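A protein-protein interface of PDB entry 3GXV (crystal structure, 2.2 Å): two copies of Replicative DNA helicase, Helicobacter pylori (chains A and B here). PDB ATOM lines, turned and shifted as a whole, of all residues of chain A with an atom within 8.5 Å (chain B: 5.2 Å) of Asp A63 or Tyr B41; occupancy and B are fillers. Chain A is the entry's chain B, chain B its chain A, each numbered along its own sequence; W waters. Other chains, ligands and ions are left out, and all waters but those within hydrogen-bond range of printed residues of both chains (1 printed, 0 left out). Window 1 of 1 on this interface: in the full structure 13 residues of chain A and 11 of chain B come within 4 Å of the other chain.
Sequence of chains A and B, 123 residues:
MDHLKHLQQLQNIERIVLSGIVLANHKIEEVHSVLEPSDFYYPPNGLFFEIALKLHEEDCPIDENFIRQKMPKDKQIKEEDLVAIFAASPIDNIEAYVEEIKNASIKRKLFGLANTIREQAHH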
ATOM      1  N   ILE A  21      -9.909 -11.257   6.410  1.00  0.00           N
ATOM      2  CA  ILE A  21      -8.517 -11.487   6.801  1.00  0.00           C
ATOM      3  C   ILE A  21      -8.031 -12.840   6.279  1.00  0.00           C
ATOM      4  O   ILE A  21      -6.849 -13.005   5.954  1.00  0.00           O
ATOM      5  CB  ILE A  21      -8.367 -11.461   8.342  1.00  0.00           C
ATOM      6  CG1 ILE A  21      -8.597 -10.039   8.853  1.00  0.00           C
ATOM      7  CG2 ILE A  21      -6.992 -12.003   8.761  1.00  0.00           C
ATOM      8  CD1 ILE A  21      -8.427  -9.896  10.346  1.00  0.00           C
ATOM      9  N   VAL A  22      -8.953 -13.798   6.204  1.00  0.00           N
ATOM     10  CA  VAL A  22      -8.642 -15.136   5.715  1.00  0.00           C
ATOM     11  C   VAL A  22      -8.372 -15.112   4.211  1.00  0.00           C
ATOM     12  O   VAL A  22      -7.654 -15.958   3.690  1.00  0.00           O
ATOM     13  CB  VAL A  22      -9.795 -16.115   6.028  1.00  0.00           C
ATOM     14  CG1 VAL A  22      -9.562 -17.453   5.337  1.00  0.00           C
ATOM     15  CG2 VAL A  22      -9.901 -16.315   7.541  1.00  0.00           C
ATOM     16  N   LEU A  23      -8.956 -14.134   3.526  1.00  0.00           N
ATOM     17  CA  LEU A  23      -8.782 -13.957   2.080  1.00  0.00           C
ATOM     18  C   LEU A  23      -7.481 -13.197   1.780  1.00  0.00           C
ATOM     19  O   LEU A  23      -6.818 -13.445   0.766  1.00  0.00           O
ATOM     20  CB  LEU A  23      -9.971 -13.193   1.498  1.00  0.00           C
ATOM     21  CG  LEU A  23      -9.698 -12.455   0.188  1.00  0.00           C
ATOM     22  CD1 LEU A  23      -9.278 -13.447  -0.889  1.00  0.00           C
ATOM     23  CD2 LEU A  23     -10.941 -11.692  -0.227  1.00  0.00           C
ATOM     24  N   ASN A  25      -4.509 -12.462   4.239  1.00  0.00           N
ATOM     25  CA  ASN A  25      -3.828 -12.540   5.535  1.00  0.00           C
ATOM     26  C   ASN A  25      -3.019 -11.288   5.895  1.00  0.00           C
ATOM     27  O   ASN A  25      -2.689 -11.067   7.060  1.00  0.00           O
ATOM     28  CB  ASN A  25      -2.930 -13.784   5.569  1.00  0.00           C
ATOM     29  CG  ASN A  25      -3.724 -15.074   5.438  1.00  0.00           C
ATOM     30  OD1 ASN A  25      -4.806 -15.087   4.858  1.00  0.00           O
ATOM     31  ND2 ASN A  25      -3.189 -16.164   5.971  1.00  0.00           N
ATOM     32  N   PHE A  48     -10.778 -16.221  17.715  1.00  0.00           N
ATOM     33  CA  PHE A  48     -10.329 -16.465  16.346  1.00  0.00           C
ATOM     34  C   PHE A  48      -9.270 -15.419  15.990  1.00  0.00           C
ATOM     35  O   PHE A  48      -8.184 -15.769  15.539  1.00  0.00           O
ATOM     36  CB  PHE A  48     -11.496 -16.343  15.365  1.00  0.00           C
ATOM     37  CG  PHE A  48     -11.151 -16.736  13.956  1.00  0.00           C
ATOM     38  CD1 PHE A  48     -11.302 -18.045  13.537  1.00  0.00           C
ATOM     39  CD2 PHE A  48     -10.699 -15.788  13.038  1.00  0.00           C
ATOM     40  CE1 PHE A  48     -11.006 -18.411  12.219  1.00  0.00           C
ATOM     41  CE2 PHE A  48     -10.402 -16.141  11.724  1.00  0.00           C
ATOM     42  CZ  PHE A  48     -10.559 -17.455  11.312  1.00  0.00           C
ATOM     43  N   ILE A  51      -5.946 -16.378  17.596  1.00  0.00           N
ATOM     44  CA  ILE A  51      -5.194 -17.448  16.954  1.00  0.00           C
ATOM     45  C   ILE A  51      -4.598 -16.950  15.642  1.00  0.00           C
ATOM     46  O   ILE A  51      -3.497 -17.352  15.255  1.00  0.00           O
ATOM     47  CB  ILE A  51      -6.086 -18.681  16.681  1.00  0.00           C
ATOM     48  CG1 ILE A  51      -6.566 -19.290  18.006  1.00  0.00           C
ATOM     49  CG2 ILE A  51      -5.302 -19.717  15.893  1.00  0.00           C
ATOM     50  CD1 ILE A  51      -7.753 -20.247  17.861  1.00  0.00           C
ATOM     51  N   ALA A  52      -5.319 -16.062  14.966  1.00  0.00           N
ATOM     52  CA  ALA A  52      -4.850 -15.522  13.698  1.00  0.00           C
ATOM     53  C   ALA A  52      -3.625 -14.652  13.935  1.00  0.00           C
ATOM     54  O   ALA A  52      -2.624 -14.776  13.233  1.00  0.00           O
ATOM     55  CB  ALA A  52      -5.958 -14.714  13.017  1.00  0.00           C
ATOM     56  N   LEU A  55      -0.795 -16.895  14.431  1.00  0.00           N
ATOM     57  CA  LEU A  55      -0.384 -17.551  13.193  1.00  0.00           C
ATOM     58  C   LEU A  55       0.385 -16.630  12.259  1.00  0.00           C
ATOM     59  O   LEU A  55       1.242 -17.082  11.507  1.00  0.00           O
ATOM     60  CB  LEU A  55      -1.599 -18.096  12.438  1.00  0.00           C
ATOM     61  CG  LEU A  55      -2.293 -19.349  12.965  1.00  0.00           C
ATOM     62  CD1 LEU A  55      -3.517 -19.662  12.096  1.00  0.00           C
ATOM     63  CD2 LEU A  55      -1.299 -20.517  12.966  1.00  0.00           C
ATOM     64  N   ASP A  59       4.358 -16.398  10.615  1.00  0.00           N
ATOM     65  CA  ASP A  59       4.279 -16.414   9.160  1.00  0.00           C
ATOM     66  C   ASP A  59       3.557 -17.649   8.624  1.00  0.00           C
ATOM     67  O   ASP A  59       3.781 -18.075   7.485  1.00  0.00           O
ATOM     68  CB  ASP A  59       5.684 -16.290   8.566  1.00  0.00           C
ATOM     69  CG  ASP A  59       6.434 -15.068   9.098  1.00  0.00           C
ATOM     70  OD1 ASP A  59       7.569 -14.800   8.655  1.00  0.00           O
ATOM     71  OD2 ASP A  59       5.881 -14.370   9.972  1.00  0.00           O
ATOM     72  N   CYS A  60       2.681 -18.221   9.448  1.00  0.00           N
ATOM     73  CA  CYS A  60       1.909 -19.386   9.031  1.00  0.00           C
ATOM     74  C   CYS A  60       0.606 -18.897   8.412  1.00  0.00           C
ATOM     75  O   CYS A  60      -0.021 -17.960   8.913  1.00  0.00           O
ATOM     76  CB  CYS A  60       1.595 -20.304  10.217  1.00  0.00           C
ATOM     77  SG  CYS A  60       0.697 -21.815   9.732  1.00  0.00           S
ATOM     78  N   PRO A  61       0.180 -19.521   7.309  1.00  0.00           N
ATOM     79  CA  PRO A  61      -1.061 -19.079   6.685  1.00  0.00           C
ATOM     80  C   PRO A  61      -2.236 -19.064   7.665  1.00  0.00           C
ATOM     81  O   PRO A  61      -2.256 -19.805   8.643  1.00  0.00           O
ATOM     82  CB  PRO A  61      -1.256 -20.096   5.562  1.00  0.00           C
ATOM     83  CG  PRO A  61       0.145 -20.478   5.189  1.00  0.00           C
ATOM     84  CD  PRO A  61       0.811 -20.607   6.533  1.00  0.00           C
ATOM     85  N   ILE A  62      -3.206 -18.194   7.411  1.00  0.00           N
ATOM     86  CA  ILE A  62      -4.390 -18.143   8.250  1.00  0.00           C
ATOM     87  C   ILE A  62      -5.500 -18.751   7.415  1.00  0.00           C
ATOM     88  O   ILE A  62      -6.093 -18.079   6.582  1.00  0.00           O
ATOM     89  CB  ILE A  62      -4.778 -16.708   8.611  1.00  0.00           C
ATOM     90  CG1 ILE A  62      -3.725 -16.115   9.545  1.00  0.00           C
ATOM     91  CG2 ILE A  62      -6.175 -16.695   9.232  1.00  0.00           C
ATOM     92  CD1 ILE A  62      -3.888 -14.620   9.810  1.00  0.00           C
ATOM     93  N   ASP A  63      -5.761 -20.035   7.617  1.00  0.00           N
ATOM     94  CA  ASP A  63      -6.802 -20.711   6.860  1.00  0.00           C
ATOM     95  C   ASP A  63      -7.553 -21.704   7.734  1.00  0.00           C
ATOM     96  O   ASP A  63      -7.258 -21.848   8.921  1.00  0.00           O
ATOM     97  CB  ASP A  63      -6.201 -21.414   5.629  1.00  0.00           C
ATOM     98  CG  ASP A  63      -5.084 -22.399   5.984  1.00  0.00           C
ATOM     99  OD1 ASP A  63      -5.290 -23.229   6.888  1.00  0.00           O
ATOM    100  OD2 ASP A  63      -4.010 -22.355   5.338  1.00  0.00           O
ATOM    101  N   GLU A  64      -8.538 -22.366   7.144  1.00  0.00           N
ATOM    102  CA  GLU A  64      -9.338 -23.343   7.862  1.00  0.00           C
ATOM    103  C   GLU A  64      -8.456 -24.388   8.549  1.00  0.00           C
ATOM    104  O   GLU A  64      -8.650 -24.692   9.734  1.00  0.00           O
ATOM    105  CB  GLU A  64     -10.307 -24.025   6.899  1.00  0.00           C
ATOM    106  CG  GLU A  64     -11.764 -23.861   7.298  1.00  0.00           C
ATOM    107  CD  GLU A  64     -12.723 -24.469   6.299  1.00  0.00           C
ATOM    108  OE1 GLU A  64     -12.653 -24.104   5.109  1.00  0.00           O
ATOM    109  OE2 GLU A  64     -13.552 -25.306   6.705  1.00  0.00           O
ATOM    110  N   ASN A  65      -7.487 -24.926   7.806  1.00  0.00           N
ATOM    111  CA  ASN A  65      -6.569 -25.941   8.335  1.00  0.00           C
ATOM    112  C   ASN A  65      -5.823 -25.478   9.578  1.00  0.00           C
ATOM    113  O   ASN A  65      -6.017 -26.020  10.655  1.00  0.00           O
ATOM    114  CB  ASN A  65      -5.562 -26.375   7.252  1.00  0.00           C
ATOM    115  CG  ASN A  65      -4.386 -27.176   7.815  1.00  0.00           C
ATOM    116  OD1 ASN A  65      -4.535 -27.931   8.770  1.00  0.00           O
ATOM    117  ND2 ASN A  65      -3.213 -27.021   7.205  1.00  0.00           N
ATOM    118  N   PHE A  66      -4.982 -24.467   9.442  1.00  0.00           N
ATOM    119  CA  PHE A  66      -4.211 -24.001  10.583  1.00  0.00           C
ATOM    120  C   PHE A  66      -4.978 -23.365  11.734  1.00  0.00           C
ATOM    121  O   PHE A  66      -4.519 -23.403  12.879  1.00  0.00           O
ATOM    122  CB  PHE A  66      -3.123 -23.075  10.083  1.00  0.00           C
ATOM    123  CG  PHE A  66      -2.137 -23.766   9.186  1.00  0.00           C
ATOM    124  CD1 PHE A  66      -1.261 -24.714   9.701  1.00  0.00           C
ATOM    125  CD2 PHE A  66      -2.120 -23.507   7.818  1.00  0.00           C
ATOM    126  CE1 PHE A  66      -0.386 -25.391   8.875  1.00  0.00           C
ATOM    127  CE2 PHE A  66      -1.247 -24.181   6.986  1.00  0.00           C
ATOM    128  CZ  PHE A  66      -0.378 -25.127   7.513  1.00  0.00           C
ATOM    129  N   ILE A  67      -6.148 -22.794  11.451  1.00  0.00           N
ATOM    130  CA  ILE A  67      -6.920 -22.176  12.518  1.00  0.00           C
ATOM    131  C   ILE A  67      -7.358 -23.277  13.455  1.00  0.00           C
ATOM    132  O   ILE A  67      -7.340 -23.112  14.668  1.00  0.00           O
ATOM    133  CB  ILE A  67      -8.170 -21.437  11.983  1.00  0.00           C
ATOM    134  CG1 ILE A  67      -7.753 -20.172  11.241  1.00  0.00           C
ATOM    135  CG2 ILE A  67      -9.098 -21.095  13.131  1.00  0.00           C
ATOM    136  CD1 ILE A  67      -7.037 -19.159  12.111  1.00  0.00           C
ATOM    137  N   ARG A  68      -7.728 -24.415  12.885  1.00  0.00           N
ATOM    138  CA  ARG A  68      -8.181 -25.538  13.685  1.00  0.00           C
ATOM    139  C   ARG A  68      -7.012 -26.273  14.326  1.00  0.00           C
ATOM    140  O   ARG A  68      -7.171 -26.907  15.368  1.00  0.00           O
ATOM    141  CB  ARG A  68      -8.986 -26.502  12.828  1.00  0.00           C
ATOM    142  CG  ARG A  68     -10.198 -25.882  12.159  1.00  0.00           C
ATOM    143  CD  ARG A  68     -11.269 -26.940  11.972  1.00  0.00           C
ATOM    144  NE  ARG A  68     -11.936 -26.882  10.677  1.00  0.00           N
ATOM    145  CZ  ARG A  68     -12.534 -25.804  10.188  1.00  0.00           C
ATOM    146  NH1 ARG A  68     -12.549 -24.675  10.881  1.00  0.00           N
ATOM    147  NH2 ARG A  68     -13.138 -25.862   9.006  1.00  0.00           N
ATOM    148  N   GLN A  69      -5.844 -26.205  13.698  1.00  0.00           N
ATOM    149  CA  GLN A  69      -4.668 -26.855  14.253  1.00  0.00           C
ATOM    150  C   GLN A  69      -4.124 -26.033  15.420  1.00  0.00           C
ATOM    151  O   GLN A  69      -3.674 -26.586  16.414  1.00  0.00           O
ATOM    152  CB  GLN A  69      -3.571 -27.007  13.189  1.00  0.00           C
ATOM    153  CG  GLN A  69      -3.724 -28.214  12.277  1.00  0.00           C
ATOM    154  CD  GLN A  69      -2.461 -28.495  11.471  1.00  0.00           C
ATOM    155  OE1 GLN A  69      -1.374 -28.622  12.032  1.00  0.00           O
ATOM    156  NE2 GLN A  69      -2.601 -28.601  10.154  1.00  0.00           N
ATOM    157  N   LYS A  70      -4.186 -24.710  15.301  1.00  0.00           N
ATOM    158  CA  LYS A  70      -3.666 -23.822  16.341  1.00  0.00           C
ATOM    159  C   LYS A  70      -4.657 -23.476  17.459  1.00  0.00           C
ATOM    160  O   LYS A  70      -4.386 -22.606  18.287  1.00  0.00           O
ATOM    161  CB  LYS A  70      -3.138 -22.530  15.711  1.00  0.00           C
ATOM    162  CG  LYS A  70      -2.036 -21.864  16.516  1.00  0.00           C
ATOM    163  CD  LYS A  70      -0.764 -22.715  16.505  1.00  0.00           C
ATOM    164  CE  LYS A  70       0.242 -22.204  17.512  1.00  0.00           C
ATOM    165  NZ  LYS A  70      -0.330 -22.249  18.885  1.00  0.00           N
ATOM    166  N   MET A  71      -5.804 -24.151  17.484  1.00  0.00           N
ATOM    167  CA  MET A  71      -6.803 -23.913  18.523  1.00  0.00           C
ATOM    168  C   MET A  71      -6.351 -24.549  19.842  1.00  0.00           C
ATOM    169  O   MET A  71      -6.073 -25.744  19.902  1.00  0.00           O
ATOM    170  CB  MET A  71      -8.156 -24.480  18.093  1.00  0.00           C
ATOM    171  CG  MET A  71      -9.162 -23.411  17.680  1.00  0.00           C
ATOM    172  SD  MET A  71     -10.804 -24.097  17.388  1.00  0.00           S
ATOM    173  CE  MET A  71     -10.967 -23.809  15.656  1.00  0.00           C
ATOM    174  N   LEU A  82     -17.147 -21.458  13.493  1.00  0.00           N
ATOM    175  CA  LEU A  82     -16.081 -21.468  12.504  1.00  0.00           C
ATOM    176  C   LEU A  82     -16.701 -21.329  11.122  1.00  0.00           C
ATOM    177  O   LEU A  82     -16.368 -20.410  10.377  1.00  0.00           O
ATOM    178  CB  LEU A  82     -15.281 -22.777  12.592  1.00  0.00           C
ATOM    179  CG  LEU A  82     -14.349 -23.006  13.792  1.00  0.00           C
ATOM    180  CD1 LEU A  82     -13.799 -24.421  13.755  1.00  0.00           C
ATOM    181  CD2 LEU A  82     -13.207 -22.004  13.766  1.00  0.00           C
ATOM    182  N   PHE A  86     -15.894 -18.646   8.222  1.00  0.00           N
ATOM    183  CA  PHE A  86     -15.392 -19.033   6.901  1.00  0.00           C
ATOM    184  C   PHE A  86     -16.380 -18.869   5.749  1.00  0.00           C
ATOM    185  O   PHE A  86     -15.972 -18.648   4.609  1.00  0.00           O
ATOM    186  CB  PHE A  86     -14.880 -20.484   6.926  1.00  0.00           C
ATOM    187  CG  PHE A  86     -13.622 -20.672   7.741  1.00  0.00           C
ATOM    188  CD1 PHE A  86     -12.433 -20.089   7.343  1.00  0.00           C
ATOM    189  CD2 PHE A  86     -13.645 -21.400   8.920  1.00  0.00           C
ATOM    190  CE1 PHE A  86     -11.277 -20.226   8.107  1.00  0.00           C
ATOM    191  CE2 PHE A  86     -12.497 -21.547   9.699  1.00  0.00           C
ATOM    192  CZ  PHE A  86     -11.309 -20.957   9.293  1.00  0.00           C
ATOM    193  N   LEU B   7      -6.448 -28.711   2.344  1.00  0.00           N
ATOM    194  CA  LEU B   7      -5.314 -28.023   2.931  1.00  0.00           C
ATOM    195  C   LEU B   7      -4.525 -28.995   3.782  1.00  0.00           C
ATOM    196  O   LEU B   7      -3.288 -28.934   3.835  1.00  0.00           O
ATOM    197  CB  LEU B   7      -5.803 -26.848   3.776  1.00  0.00           C
ATOM    198  CG  LEU B   7      -6.721 -25.860   3.042  1.00  0.00           C
ATOM    199  CD1 LEU B   7      -7.168 -24.751   3.992  1.00  0.00           C
ATOM    200  CD2 LEU B   7      -5.983 -25.281   1.858  1.00  0.00           C
ATOM    201  N   LEU B  10      -2.528 -31.177   1.496  1.00  0.00           N
ATOM    202  CA  LEU B  10      -1.393 -30.515   0.857  1.00  0.00           C
ATOM    203  C   LEU B  10      -0.248 -30.611   1.865  1.00  0.00           C
ATOM    204  O   LEU B  10       0.902 -30.826   1.498  1.00  0.00           O
ATOM    205  CB  LEU B  10      -1.700 -29.034   0.603  1.00  0.00           C
ATOM    206  CG  LEU B  10      -1.090 -28.302  -0.606  1.00  0.00           C
ATOM    207  CD1 LEU B  10      -1.292 -26.814  -0.401  1.00  0.00           C
ATOM    208  CD2 LEU B  10       0.388 -28.605  -0.784  1.00  0.00           C
ATOM    209  N   GLN B  11      -0.587 -30.443   3.141  1.00  0.00           N
ATOM    210  CA  GLN B  11       0.395 -30.504   4.215  1.00  0.00           C
ATOM    211  C   GLN B  11       0.985 -31.905   4.328  1.00  0.00           C
ATOM    212  O   GLN B  11       2.192 -32.077   4.500  1.00  0.00           O
ATOM    213  CB  GLN B  11      -0.243 -30.122   5.546  1.00  0.00           C
ATOM    214  CG  GLN B  11       0.619 -29.182   6.360  1.00  0.00           C
ATOM    215  CD  GLN B  11       0.157 -29.062   7.787  1.00  0.00           C
ATOM    216  OE1 GLN B  11      -1.034 -28.889   8.055  1.00  0.00           O
ATOM    217  NE2 GLN B  11       1.098 -29.142   8.718  1.00  0.00           N
ATOM    218  N   GLU B  14       3.317 -32.710   1.285  1.00  0.00           N
ATOM    219  CA  GLU B  14       4.659 -32.127   1.374  1.00  0.00           C
ATOM    220  C   GLU B  14       5.572 -33.004   2.248  1.00  0.00           C
ATOM    221  O   GLU B  14       6.736 -33.264   1.891  1.00  0.00           O
ATOM    222  CB  GLU B  14       4.585 -30.686   1.913  1.00  0.00           C
ATOM    223  CG  GLU B  14       3.672 -29.797   1.054  1.00  0.00           C
ATOM    224  CD  GLU B  14       3.700 -28.325   1.424  1.00  0.00           C
ATOM    225  OE1 GLU B  14       3.975 -27.982   2.597  1.00  0.00           O
ATOM    226  OE2 GLU B  14       3.423 -27.512   0.524  1.00  0.00           O
ATOM    227  N   ASP B  39       7.749 -22.538  -2.603  1.00  0.00           N
ATOM    228  CA  ASP B  39       6.531 -23.194  -3.078  1.00  0.00           C
ATOM    229  C   ASP B  39       5.802 -24.040  -2.045  1.00  0.00           C
ATOM    230  O   ASP B  39       4.712 -24.536  -2.308  1.00  0.00           O
ATOM    231  CB  ASP B  39       6.845 -24.067  -4.286  1.00  0.00           C
ATOM    232  CG  ASP B  39       7.294 -23.253  -5.474  1.00  0.00           C
ATOM    233  OD1 ASP B  39       6.505 -22.390  -5.916  1.00  0.00           O
ATOM    234  OD2 ASP B  39       8.424 -23.478  -5.954  1.00  0.00           O
ATOM    235  N   PHE B  40       6.396 -24.217  -0.880  1.00  0.00           N
ATOM    236  CA  PHE B  40       5.763 -25.019   0.146  1.00  0.00           C
ATOM    237  C   PHE B  40       4.725 -24.273   0.986  1.00  0.00           C
ATOM    238  O   PHE B  40       4.980 -23.198   1.529  1.00  0.00           O
ATOM    239  CB  PHE B  40       6.825 -25.643   1.051  1.00  0.00           C
ATOM    240  CG  PHE B  40       7.530 -26.811   0.430  1.00  0.00           C
ATOM    241  CD1 PHE B  40       7.067 -28.108   0.633  1.00  0.00           C
ATOM    242  CD2 PHE B  40       8.649 -26.621  -0.367  1.00  0.00           C
ATOM    243  CE1 PHE B  40       7.716 -29.195   0.050  1.00  0.00           C
ATOM    244  CE2 PHE B  40       9.305 -27.707  -0.957  1.00  0.00           C
ATOM    245  CZ  PHE B  40       8.840 -28.991  -0.747  1.00  0.00           C
ATOM    246  N   TYR B  41       3.551 -24.892   1.068  1.00  0.00           N
ATOM    247  CA  TYR B  41       2.396 -24.419   1.818  1.00  0.00           C
ATOM    248  C   TYR B  41       2.708 -24.200   3.299  1.00  0.00           C
ATOM    249  O   TYR B  41       2.475 -23.111   3.845  1.00  0.00           O
ATOM    250  CB  TYR B  41       1.279 -25.453   1.659  1.00  0.00           C
ATOM    251  CG  TYR B  41       0.074 -25.264   2.549  1.00  0.00           C
ATOM    252  CD1 TYR B  41      -0.624 -24.051   2.579  1.00  0.00           C
ATOM    253  CD2 TYR B  41      -0.395 -26.319   3.339  1.00  0.00           C
ATOM    254  CE1 TYR B  41      -1.763 -23.904   3.366  1.00  0.00           C
ATOM    255  CE2 TYR B  41      -1.532 -26.182   4.124  1.00  0.00           C
ATOM    256  CZ  TYR B  41      -2.204 -24.974   4.134  1.00  0.00           C
ATOM    257  OH  TYR B  41      -3.323 -24.863   4.905  1.00  0.00           O
ATOM    258  N   TYR B  42       3.200 -25.249   3.951  1.00  0.00           N
ATOM    259  CA  TYR B  42       3.569 -25.177   5.363  1.00  0.00           C
ATOM    260  C   TYR B  42       5.025 -24.730   5.396  1.00  0.00           C
ATOM    261  O   TYR B  42       5.917 -25.477   4.983  1.00  0.00           O
ATOM    262  CB  TYR B  42       3.400 -26.552   6.009  1.00  0.00           C
ATOM    263  CG  TYR B  42       3.576 -26.550   7.510  1.00  0.00           C
ATOM    264  CD1 TYR B  42       2.881 -25.636   8.306  1.00  0.00           C
ATOM    265  CD2 TYR B  42       4.375 -27.500   8.140  1.00  0.00           C
ATOM    266  CE1 TYR B  42       2.977 -25.665   9.702  1.00  0.00           C
ATOM    267  CE2 TYR B  42       4.478 -27.540   9.530  1.00  0.00           C
ATOM    268  CZ  TYR B  42       3.767 -26.619  10.303  1.00  0.00           C
ATOM    269  OH  TYR B  42       3.853 -26.639  11.674  1.00  0.00           O
ATOM    270  N   PRO B  43       5.286 -23.507   5.898  1.00  0.00           N
ATOM    271  CA  PRO B  43       6.632 -22.917   5.982  1.00  0.00           C
ATOM    272  C   PRO B  43       7.766 -23.802   6.480  1.00  0.00           C
ATOM    273  O   PRO B  43       8.846 -23.806   5.887  1.00  0.00           O
ATOM    274  CB  PRO B  43       6.410 -21.671   6.850  1.00  0.00           C
ATOM    275  CG  PRO B  43       4.975 -21.293   6.510  1.00  0.00           C
ATOM    276  CD  PRO B  43       4.317 -22.648   6.604  1.00  0.00           C
ATOM    277  N   ARG B 108      -1.782 -19.892  -4.833  1.00  0.00           N
ATOM    278  CA  ARG B 108      -1.571 -18.924  -3.747  1.00  0.00           C
ATOM    279  C   ARG B 108      -0.991 -17.609  -4.254  1.00  0.00           C
ATOM    280  O   ARG B 108      -1.434 -16.534  -3.847  1.00  0.00           O
ATOM    281  CB  ARG B 108      -0.652 -19.491  -2.651  1.00  0.00           C
ATOM    282  CG  ARG B 108      -1.300 -20.514  -1.713  1.00  0.00           C
ATOM    283  CD  ARG B 108      -0.434 -20.769  -0.475  1.00  0.00           C
ATOM    284  NE  ARG B 108       0.893 -21.290  -0.819  1.00  0.00           N
ATOM    285  CZ  ARG B 108       1.146 -22.532  -1.238  1.00  0.00           C
ATOM    286  NH1 ARG B 108       0.170 -23.424  -1.368  1.00  0.00           N
ATOM    287  NH2 ARG B 108       2.389 -22.877  -1.552  1.00  0.00           N
HETATM  288  O   HOH W   1      -3.320 -31.049   8.109  1.00  0.00           O
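The side-chain amide oxygen (OE1) of Gln B11 lies within hydrogen-bond range of the side-chain amide nitrogen (ND2) of Asn A65, 3.0 Å away.
The side-chain amide nitrogen of Gln A69 sits at hydrogen-bond distance from the side-chain amide oxygen of Gln B11, at 2.6 Å.
OD2 of Asp A63 sits at hydrogen-bond distance from OH of Tyr B41.
The side-chain hydroxyl of Tyr B41 sits at hydrogen-bond distance from the side-chain amide nitrogen of Asn A65, at 3.2 Å.
OE2 of Glu B14 is in hydrogen-bond range of N of Tyr B41, at 2.7 Å.
OE1 of Glu B14 lies within hydrogen-bond range of N of Tyr B42 (3.1 Å).
The side-chain carboxylate of Asp A63 sits at hydrogen-bond distance from the backbone NH of Asn A65 (2.9 Å).
OD1 of Asp A63 is in hydrogen-bond range of N of Phe A66, 2.9 Å away.
OD1 of Asn A65 is in hydrogen-bond range of NE2 of Gln A69 (2.5 Å).
Pro B43 touches Asp A59.
Tyr B41 touches Pro A61 (O to CG, 3.8 Å).
Asp A63 touches Leu B7.
Asn A65 touches Leu B7.
OE1 of Gln B11 touches CE1 of Phe A66, 3.7 Å away.
OH of Tyr B41 touches CE2 of Phe A66, at 3.0 Å.
Phe A66 touches Tyr B42.
Of chain B, only Leu B7 (3.7 Å) and Tyr B41 (2.6 Å) come within 4 Å of Asp A63.
Of chain A, only Pro A61 (3.8 Å), Asp A63 (2.6 Å), Asn A65 (3.2 Å) and Phe A66 (3.0 Å) come within 4 Å of Tyr B41.
Printed residues of chain A within 4 Å of Pro B43: Asp A59 (3.6 Å).
Of the printed residues of chain A, Leu B7 touches Asp A63 and Asn A65.
Arg A68 touches none of the printed residues of chain B.
Phe B40 touches none of the printed residues of chain A.
The nearest printed residue of chain B that does not touch Asp A63 is Arg B108 (7.0 Å).
Of the 10 printed residues of chain B, 5 touch a printed residue of chain A.
Hydrophobic or aromatic side chains of chain B within 4 Å of the printed part of chain A: Leu B7, Tyr B41, Tyr B42 and Pro B43.
Along chain B the printed residues that touch a printed residue of chain A span positions 7 to 43.
Of the 23 printed residues of chain A, 6 touch a printed residue of chain B.
Printed residues of chain A that touch a printed residue of chain B: Asp A59, Pro A61, Asp A63, Asn A65, Phe A66 and Gln A69.
Hydrophobic or aromatic side chains of chain A that line the printed part of chain B: Pro A61 and Phe A66.
Among the printed residues, 11 pairs touch across the chains.
No position is printed for both chains.
Of the 11 pairs that touch across the chains among the printed residues, none has its exchanged pair printed and touching as well.
Water W1 lies within hydrogen-bond range of the side-chain amide oxygen (OE1) of Gln B11, the side-chain amide nitrogen (NE2) of Gln A69 and the side-chain amide oxygen (OD1) of Asn A65.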
